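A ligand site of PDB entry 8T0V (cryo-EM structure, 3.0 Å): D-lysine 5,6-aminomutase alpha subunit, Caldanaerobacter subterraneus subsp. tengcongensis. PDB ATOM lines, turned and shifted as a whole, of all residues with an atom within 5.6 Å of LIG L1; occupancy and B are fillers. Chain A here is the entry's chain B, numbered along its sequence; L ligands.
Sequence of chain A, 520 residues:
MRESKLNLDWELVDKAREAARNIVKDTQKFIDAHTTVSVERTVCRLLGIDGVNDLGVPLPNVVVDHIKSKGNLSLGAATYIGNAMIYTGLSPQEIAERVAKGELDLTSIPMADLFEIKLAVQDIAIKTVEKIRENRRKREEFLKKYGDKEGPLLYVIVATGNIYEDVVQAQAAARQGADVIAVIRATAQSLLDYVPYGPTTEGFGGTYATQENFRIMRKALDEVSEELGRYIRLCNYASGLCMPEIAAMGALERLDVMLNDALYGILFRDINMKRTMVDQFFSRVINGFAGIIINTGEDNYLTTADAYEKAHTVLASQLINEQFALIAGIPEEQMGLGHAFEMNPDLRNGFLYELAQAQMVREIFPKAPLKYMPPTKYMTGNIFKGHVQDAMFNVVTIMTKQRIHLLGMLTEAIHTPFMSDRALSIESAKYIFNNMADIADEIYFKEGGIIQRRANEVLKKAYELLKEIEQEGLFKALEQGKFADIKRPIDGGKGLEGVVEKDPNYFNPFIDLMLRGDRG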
ATOM      1  N   TYR A 155       2.399 -15.548  -9.570  1.00  0.00           N
ATOM      2  CA  TYR A 155       2.386 -16.851  -8.908  1.00  0.00           C
ATOM      3  C   TYR A 155       3.745 -17.492  -9.113  1.00  0.00           C
ATOM      4  O   TYR A 155       4.090 -17.878 -10.236  1.00  0.00           O
ATOM      5  CB  TYR A 155       1.248 -17.706  -9.488  1.00  0.00           C
ATOM      6  CG  TYR A 155       1.024 -19.070  -8.882  1.00  0.00           C
ATOM      7  CD1 TYR A 155       2.057 -20.001  -8.802  1.00  0.00           C
ATOM      8  CD2 TYR A 155      -0.219 -19.445  -8.428  1.00  0.00           C
ATOM      9  CE1 TYR A 155       1.841 -21.241  -8.261  1.00  0.00           C
ATOM     10  CE2 TYR A 155      -0.435 -20.685  -7.888  1.00  0.00           C
ATOM     11  CZ  TYR A 155       0.604 -21.579  -7.810  1.00  0.00           C
ATOM     12  OH  TYR A 155       0.405 -22.833  -7.276  1.00  0.00           O
ATOM     13  N   ILE A 157       6.853 -20.307  -7.539  1.00  0.00           N
ATOM     14  CA  ILE A 157       7.025 -21.593  -6.871  1.00  0.00           C
ATOM     15  C   ILE A 157       8.423 -21.633  -6.276  1.00  0.00           C
ATOM     16  O   ILE A 157       9.395 -21.239  -6.930  1.00  0.00           O
ATOM     17  CB  ILE A 157       6.819 -22.776  -7.829  1.00  0.00           C
ATOM     18  CG1 ILE A 157       5.353 -22.855  -8.273  1.00  0.00           C
ATOM     19  CG2 ILE A 157       7.229 -24.079  -7.181  1.00  0.00           C
ATOM     20  CD1 ILE A 157       5.147 -23.689  -9.506  1.00  0.00           C
ATOM     21  N   ILE A 184       6.200 -26.373  -4.185  1.00  0.00           N
ATOM     22  CA  ILE A 184       6.024 -27.618  -4.930  1.00  0.00           C
ATOM     23  C   ILE A 184       6.428 -28.790  -4.048  1.00  0.00           C
ATOM     24  O   ILE A 184       7.398 -28.718  -3.292  1.00  0.00           O
ATOM     25  CB  ILE A 184       6.834 -27.582  -6.229  1.00  0.00           C
ATOM     26  CG1 ILE A 184       6.403 -28.722  -7.163  1.00  0.00           C
ATOM     27  CG2 ILE A 184       8.312 -27.703  -5.945  1.00  0.00           C
ATOM     28  CD1 ILE A 184       5.089 -28.477  -7.864  1.00  0.00           C
ATOM     29  N   TYR A 237      -0.608 -28.618  -2.683  1.00  0.00           N
ATOM     30  CA  TYR A 237      -1.186 -29.613  -3.573  1.00  0.00           C
ATOM     31  C   TYR A 237      -1.832 -30.698  -2.740  1.00  0.00           C
ATOM     32  O   TYR A 237      -1.208 -31.274  -1.849  1.00  0.00           O
ATOM     33  CB  TYR A 237      -0.110 -30.194  -4.493  1.00  0.00           C
ATOM     34  CG  TYR A 237       0.690 -29.134  -5.207  1.00  0.00           C
ATOM     35  CD1 TYR A 237       1.666 -28.405  -4.560  1.00  0.00           C
ATOM     36  CD2 TYR A 237       0.436 -28.850  -6.541  1.00  0.00           C
ATOM     37  CE1 TYR A 237       2.369 -27.421  -5.209  1.00  0.00           C
ATOM     38  CE2 TYR A 237       1.138 -27.872  -7.198  1.00  0.00           C
ATOM     39  CZ  TYR A 237       2.110 -27.168  -6.532  1.00  0.00           C
ATOM     40  OH  TYR A 237       2.816 -26.183  -7.195  1.00  0.00           O
ATOM     41  N   LEU A 259      -4.277 -27.144  -5.028  1.00  0.00           N
ATOM     42  CA  LEU A 259      -4.394 -27.821  -6.320  1.00  0.00           C
ATOM     43  C   LEU A 259      -5.121 -29.138  -6.129  1.00  0.00           C
ATOM     44  O   LEU A 259      -4.536 -30.123  -5.663  1.00  0.00           O
ATOM     45  CB  LEU A 259      -3.021 -28.036  -6.934  1.00  0.00           C
ATOM     46  CG  LEU A 259      -2.536 -26.911  -7.858  1.00  0.00           C
ATOM     47  CD1 LEU A 259      -1.814 -25.839  -7.069  1.00  0.00           C
ATOM     48  CD2 LEU A 259      -1.648 -27.476  -8.945  1.00  0.00           C
ATOM     49  N   GLY A 297      -5.737 -28.956 -13.170  1.00  0.00           N
ATOM     50  CA  GLY A 297      -4.477 -29.145 -13.877  1.00  0.00           C
ATOM     51  C   GLY A 297      -4.568 -29.582 -15.322  1.00  0.00           C
ATOM     52  O   GLY A 297      -3.841 -30.503 -15.726  1.00  0.00           O
ATOM     53  N   ASP A 299      -3.424 -28.063 -17.702  1.00  0.00           N
ATOM     54  CA  ASP A 299      -2.173 -27.714 -18.365  1.00  0.00           C
ATOM     55  C   ASP A 299      -1.374 -28.968 -18.698  1.00  0.00           C
ATOM     56  O   ASP A 299      -0.657 -29.006 -19.708  1.00  0.00           O
ATOM     57  CB  ASP A 299      -1.327 -26.809 -17.475  1.00  0.00           C
ATOM     58  CG  ASP A 299      -1.355 -27.222 -16.006  1.00  0.00           C
ATOM     59  OD1 ASP A 299      -2.404 -27.065 -15.352  1.00  0.00           O
ATOM     60  OD2 ASP A 299      -0.316 -27.697 -15.501  1.00  0.00           O
ATOM     61  N   ASN A 300      -1.475 -29.995 -17.849  1.00  0.00           N
ATOM     62  CA  ASN A 300      -0.621 -31.168 -18.003  1.00  0.00           C
ATOM     63  C   ASN A 300      -1.009 -32.005 -19.204  1.00  0.00           C
ATOM     64  O   ASN A 300      -0.211 -32.812 -19.681  1.00  0.00           O
ATOM     65  CB  ASN A 300      -0.687 -32.012 -16.730  1.00  0.00           C
ATOM     66  CG  ASN A 300      -0.145 -31.294 -15.520  1.00  0.00           C
ATOM     67  OD1 ASN A 300       1.061 -31.054 -15.404  1.00  0.00           O
ATOM     68  ND2 ASN A 300      -1.030 -30.922 -14.609  1.00  0.00           N
ATOM     69  N   THR A 303       1.295 -31.342 -22.389  1.00  0.00           N
ATOM     70  CA  THR A 303       2.677 -31.797 -22.394  1.00  0.00           C
ATOM     71  C   THR A 303       2.820 -33.218 -22.926  1.00  0.00           C
ATOM     72  O   THR A 303       3.937 -33.639 -23.244  1.00  0.00           O
ATOM     73  CB  THR A 303       3.269 -31.719 -20.987  1.00  0.00           C
ATOM     74  OG1 THR A 303       2.681 -32.728 -20.160  1.00  0.00           O
ATOM     75  CG2 THR A 303       3.017 -30.349 -20.368  1.00  0.00           C
ATOM     76  N   ALA A 340      -3.210 -23.499 -20.362  1.00  0.00           N
ATOM     77  CA  ALA A 340      -1.823 -23.125 -20.575  1.00  0.00           C
ATOM     78  C   ALA A 340      -1.619 -22.582 -21.979  1.00  0.00           C
ATOM     79  O   ALA A 340      -2.380 -22.879 -22.899  1.00  0.00           O
ATOM     80  CB  ALA A 340      -0.890 -24.333 -20.333  1.00  0.00           C
ATOM     81  N   GLU A 342       0.326 -23.157 -24.729  1.00  0.00           N
ATOM     82  CA  GLU A 342       1.096 -24.367 -25.012  1.00  0.00           C
ATOM     83  C   GLU A 342       0.975 -24.821 -26.462  1.00  0.00           C
ATOM     84  O   GLU A 342       0.758 -26.008 -26.713  1.00  0.00           O
ATOM     85  CB  GLU A 342       0.666 -25.488 -24.066  1.00  0.00           C
ATOM     86  CG  GLU A 342       1.482 -25.576 -22.795  1.00  0.00           C
ATOM     87  CD  GLU A 342       2.792 -26.297 -22.994  1.00  0.00           C
ATOM     88  OE1 GLU A 342       3.383 -26.143 -24.074  1.00  0.00           O
ATOM     89  OE2 GLU A 342       3.218 -27.009 -22.072  1.00  0.00           O
ATOM     90  N   LYS A 371      -6.941 -19.583 -14.074  1.00  0.00           N
ATOM     91  CA  LYS A 371      -5.491 -19.636 -13.996  1.00  0.00           C
ATOM     92  C   LYS A 371      -4.907 -19.892 -15.382  1.00  0.00           C
ATOM     93  O   LYS A 371      -5.413 -20.748 -16.113  1.00  0.00           O
ATOM     94  CB  LYS A 371      -5.045 -20.724 -13.022  1.00  0.00           C
ATOM     95  CG  LYS A 371      -3.566 -20.744 -12.736  1.00  0.00           C
ATOM     96  CD  LYS A 371      -3.217 -21.856 -11.784  1.00  0.00           C
ATOM     97  CE  LYS A 371      -1.726 -22.018 -11.624  1.00  0.00           C
ATOM     98  NZ  LYS A 371      -1.391 -23.179 -10.772  1.00  0.00           N
ATOM     99  N   MET A 373      -1.156 -20.663 -17.360  1.00  0.00           N
ATOM    100  CA  MET A 373       0.147 -21.194 -17.004  1.00  0.00           C
ATOM    101  C   MET A 373       1.088 -21.193 -18.208  1.00  0.00           C
ATOM    102  O   MET A 373       0.637 -21.202 -19.360  1.00  0.00           O
ATOM    103  CB  MET A 373       0.012 -22.615 -16.441  1.00  0.00           C
ATOM    104  CG  MET A 373      -0.989 -22.692 -15.330  1.00  0.00           C
ATOM    105  SD  MET A 373      -1.490 -24.363 -14.927  1.00  0.00           S
ATOM    106  CE  MET A 373      -3.183 -24.312 -15.497  1.00  0.00           C
ATOM    107  N   PRO A 374       2.401 -21.177 -17.971  1.00  0.00           N
ATOM    108  CA  PRO A 374       3.342 -20.786 -19.016  1.00  0.00           C
ATOM    109  C   PRO A 374       3.589 -21.907 -20.014  1.00  0.00           C
ATOM    110  O   PRO A 374       3.060 -23.018 -19.856  1.00  0.00           O
ATOM    111  CB  PRO A 374       4.617 -20.456 -18.231  1.00  0.00           C
ATOM    112  CG  PRO A 374       4.531 -21.310 -17.033  1.00  0.00           C
ATOM    113  CD  PRO A 374       3.082 -21.410 -16.689  1.00  0.00           C
ATOM    114  N   PRO A 375       4.352 -21.639 -21.068  1.00  0.00           N
ATOM    115  CA  PRO A 375       4.786 -22.719 -21.964  1.00  0.00           C
ATOM    116  C   PRO A 375       5.909 -23.539 -21.345  1.00  0.00           C
ATOM    117  O   PRO A 375       6.849 -22.994 -20.770  1.00  0.00           O
ATOM    118  CB  PRO A 375       5.257 -21.975 -23.213  1.00  0.00           C
ATOM    119  CG  PRO A 375       5.650 -20.623 -22.722  1.00  0.00           C
ATOM    120  CD  PRO A 375       4.770 -20.309 -21.558  1.00  0.00           C
ATOM    121  N   THR A 376       5.783 -24.858 -21.459  1.00  0.00           N
ATOM    122  CA  THR A 376       6.802 -25.747 -20.903  1.00  0.00           C
ATOM    123  C   THR A 376       7.315 -26.731 -21.938  1.00  0.00           C
ATOM    124  O   THR A 376       8.517 -27.012 -21.987  1.00  0.00           O
ATOM    125  CB  THR A 376       6.240 -26.510 -19.720  1.00  0.00           C
ATOM    126  OG1 THR A 376       7.307 -27.203 -19.052  1.00  0.00           O
ATOM    127  CG2 THR A 376       5.219 -27.524 -20.214  1.00  0.00           C
ATOM    128  N   LEU A 406       0.566 -17.822 -13.592  1.00  0.00           N
ATOM    129  CA  LEU A 406       1.728 -18.625 -13.195  1.00  0.00           C
ATOM    130  C   LEU A 406       2.912 -18.166 -14.022  1.00  0.00           C
ATOM    131  O   LEU A 406       2.984 -18.416 -15.226  1.00  0.00           O
ATOM    132  CB  LEU A 406       1.446 -20.105 -13.382  1.00  0.00           C
ATOM    133  CG  LEU A 406       2.352 -21.045 -12.574  1.00  0.00           C
ATOM    134  CD1 LEU A 406       1.524 -22.135 -11.945  1.00  0.00           C
ATOM    135  CD2 LEU A 406       3.432 -21.649 -13.416  1.00  0.00           C
ATOM    136  N   GLU A 412      13.316 -22.626 -17.811  1.00  0.00           N
ATOM    137  CA  GLU A 412      12.470 -23.772 -17.512  1.00  0.00           C
ATOM    138  C   GLU A 412      13.104 -25.073 -17.973  1.00  0.00           C
ATOM    139  O   GLU A 412      13.094 -26.069 -17.231  1.00  0.00           O
ATOM    140  CB  GLU A 412      11.102 -23.610 -18.178  1.00  0.00           C
ATOM    141  CG  GLU A 412      10.178 -22.625 -17.471  1.00  0.00           C
ATOM    142  CD  GLU A 412       8.758 -22.670 -18.013  1.00  0.00           C
ATOM    143  OE1 GLU A 412       8.131 -23.746 -17.943  1.00  0.00           O
ATOM    144  OE2 GLU A 412       8.279 -21.632 -18.517  1.00  0.00           O
HETATM  145  N1  LIG L   1       3.331 -25.296 -17.685  1.00  0.00           N
HETATM  146  C1  LIG L   1       2.369 -25.953 -17.033  1.00  0.00           C
HETATM  147  N2  LIG L   1       2.302 -26.145 -15.713  1.00  0.00           N
HETATM  148  C2  LIG L   1       3.331 -25.716 -15.001  1.00  0.00           C
HETATM  149  N3  LIG L   1       3.527 -25.718 -13.655  1.00  0.00           N
HETATM  150  C3  LIG L   1       4.835 -25.230 -13.517  1.00  0.00           C
HETATM  151  N4  LIG L   1       5.339 -24.729 -14.662  1.00  0.00           N
HETATM  152  C4  LIG L   1       4.390 -25.094 -15.564  1.00  0.00           C
HETATM  153  C5  LIG L   1       4.326 -24.882 -16.929  1.00  0.00           C
HETATM  154  N5  LIG L   1       5.164 -24.117 -17.616  1.00  0.00           N
HETATM  155  C6  LIG L   1       2.479 -25.447 -12.683  1.00  0.00           C
HETATM  156  C7  LIG L   1       1.453 -26.567 -12.335  1.00  0.00           C
HETATM  157  C8  LIG L   1       1.321 -26.403 -10.803  1.00  0.00           C
HETATM  158  C9  LIG L   1       2.748 -26.040 -10.416  1.00  0.00           C
HETATM  159  C10 LIG L   1       3.713 -27.230 -10.434  1.00  0.00           C
HETATM  160  O1  LIG L   1       3.115 -25.114 -11.432  1.00  0.00           O
HETATM  161  O2  LIG L   1       0.199 -26.471 -13.006  1.00  0.00           O
HETATM  162  O3  LIG L   1       0.527 -25.271 -10.409  1.00  0.00           O
HETATM  163  C1  LG2 L   2      -3.058 -30.780 -10.850  1.00  0.00           C
HETATM  164  C2  LG2 L   2       6.209 -29.434 -14.756  1.00  0.00           C
HETATM  165  C3  LG2 L   2       6.280 -28.298 -15.813  1.00  0.00           C
HETATM  166  C4  LG2 L   2       7.597 -27.408 -15.678  1.00  0.00           C
HETATM  167  C5  LG2 L   2      -0.590 -30.852 -10.513  1.00  0.00           C
HETATM  168  C6  LG2 L   2      -1.855 -31.089  -9.977  1.00  0.00           C
HETATM  169  C7  LG2 L   2      -0.992 -31.803  -8.042  1.00  0.00           C
HETATM  170  C8  LG2 L   2       0.304 -31.719  -8.489  1.00  0.00           C
HETATM  171  C9  LG2 L   2       1.338 -32.120  -7.447  1.00  0.00           C
HETATM  172  C10 LG2 L   2       0.507 -31.198  -9.752  1.00  0.00           C
HETATM  173  C11 LG2 L   2       1.788 -31.048 -10.179  1.00  0.00           C
HETATM  174  C12 LG2 L   2       3.628 -30.529 -11.570  1.00  0.00           C
HETATM  175  C13 LG2 L   2       3.926 -29.954 -12.995  1.00  0.00           C
HETATM  176  N1  LG2 L   2      -2.038 -31.532  -8.776  1.00  0.00           N
HETATM  177  N2  LG2 L   2       2.168 -30.600 -11.332  1.00  0.00           N
HETATM  178  N3  LG2 L   2       6.050 -28.864 -17.246  1.00  0.00           N
HETATM  179  O1  LG2 L   2       2.047 -33.279  -7.877  1.00  0.00           O
HETATM  180  O2  LG2 L   2       1.094 -35.241  -6.566  1.00  0.00           O
HETATM  181  O3  LG2 L   2       2.775 -33.988  -5.537  1.00  0.00           O
HETATM  182  O4  LG2 L   2       3.352 -35.380  -7.397  1.00  0.00           O
HETATM  183  O5  LG2 L   2       8.126 -27.022 -16.708  1.00  0.00           O
HETATM  184  O6  LG2 L   2       7.999 -27.063 -14.579  1.00  0.00           O
HETATM  185  O7  LG2 L   2      -0.429 -30.318 -11.738  1.00  0.00           O
HETATM  186  P1  LG2 L   2       2.316 -34.475  -6.857  1.00  0.00           P
HETATM  187  S1  LG2 L   2       5.531 -28.987 -13.071  1.00  0.00           S
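An oxygen (O2) of LIG L1 is in hydrogen-bond range of the side-chain carboxylate (OD2) of Asp 299 (2.8 Å). NZ of Lys 371 lies within hydrogen-bond range of O3 of LIG L1 (2.9 Å). N5 of LIG L1 lies close to O of Pro 374 (3.3 Å). OE1 of Glu 412 sits at hydrogen-bond distance from N5 of LIG L1 (3.0 Å). O2 of LIG L1 is in hydrogen-bond range of SD of Met 373 (3.3 Å). The side-chain hydroxyl (OG1) of Thr 376 is in hydrogen-bond range of an oxygen (O5) of LG2 L2, 2.5 Å away. The side-chain amide nitrogen (ND2) of Asn 300 is in hydrogen-bond range of an oxygen (O7) of LG2 L2, at 3.0 Å.
OD2 of Asp 299 is in hydrogen-bond range of ND2 of Asn 300 (3.4 Å). The backbone NH (N) of Thr 376 lies close to the side-chain carboxylate (OE2) of Glu 342 (3.4 Å).
Residues that only touch LIG L1: Ile 157 (3.1 Å), Ile 184 (3.2 Å), Tyr 237 (3.2 Å), Thr 376 (3.4 Å), Leu 406 (3.4 Å), Leu 259 (3.4 Å), Pro 375 (3.7 Å) and Tyr 155 (3.97 Å). Within 4 Å of LIG L1: Tyr 155, Ile 157, Ile 184, Tyr 237, Leu 259, Asp 299, Lys 371, Met 373, Pro 374, Pro 375, Thr 376, Leu 406 and Glu 412.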
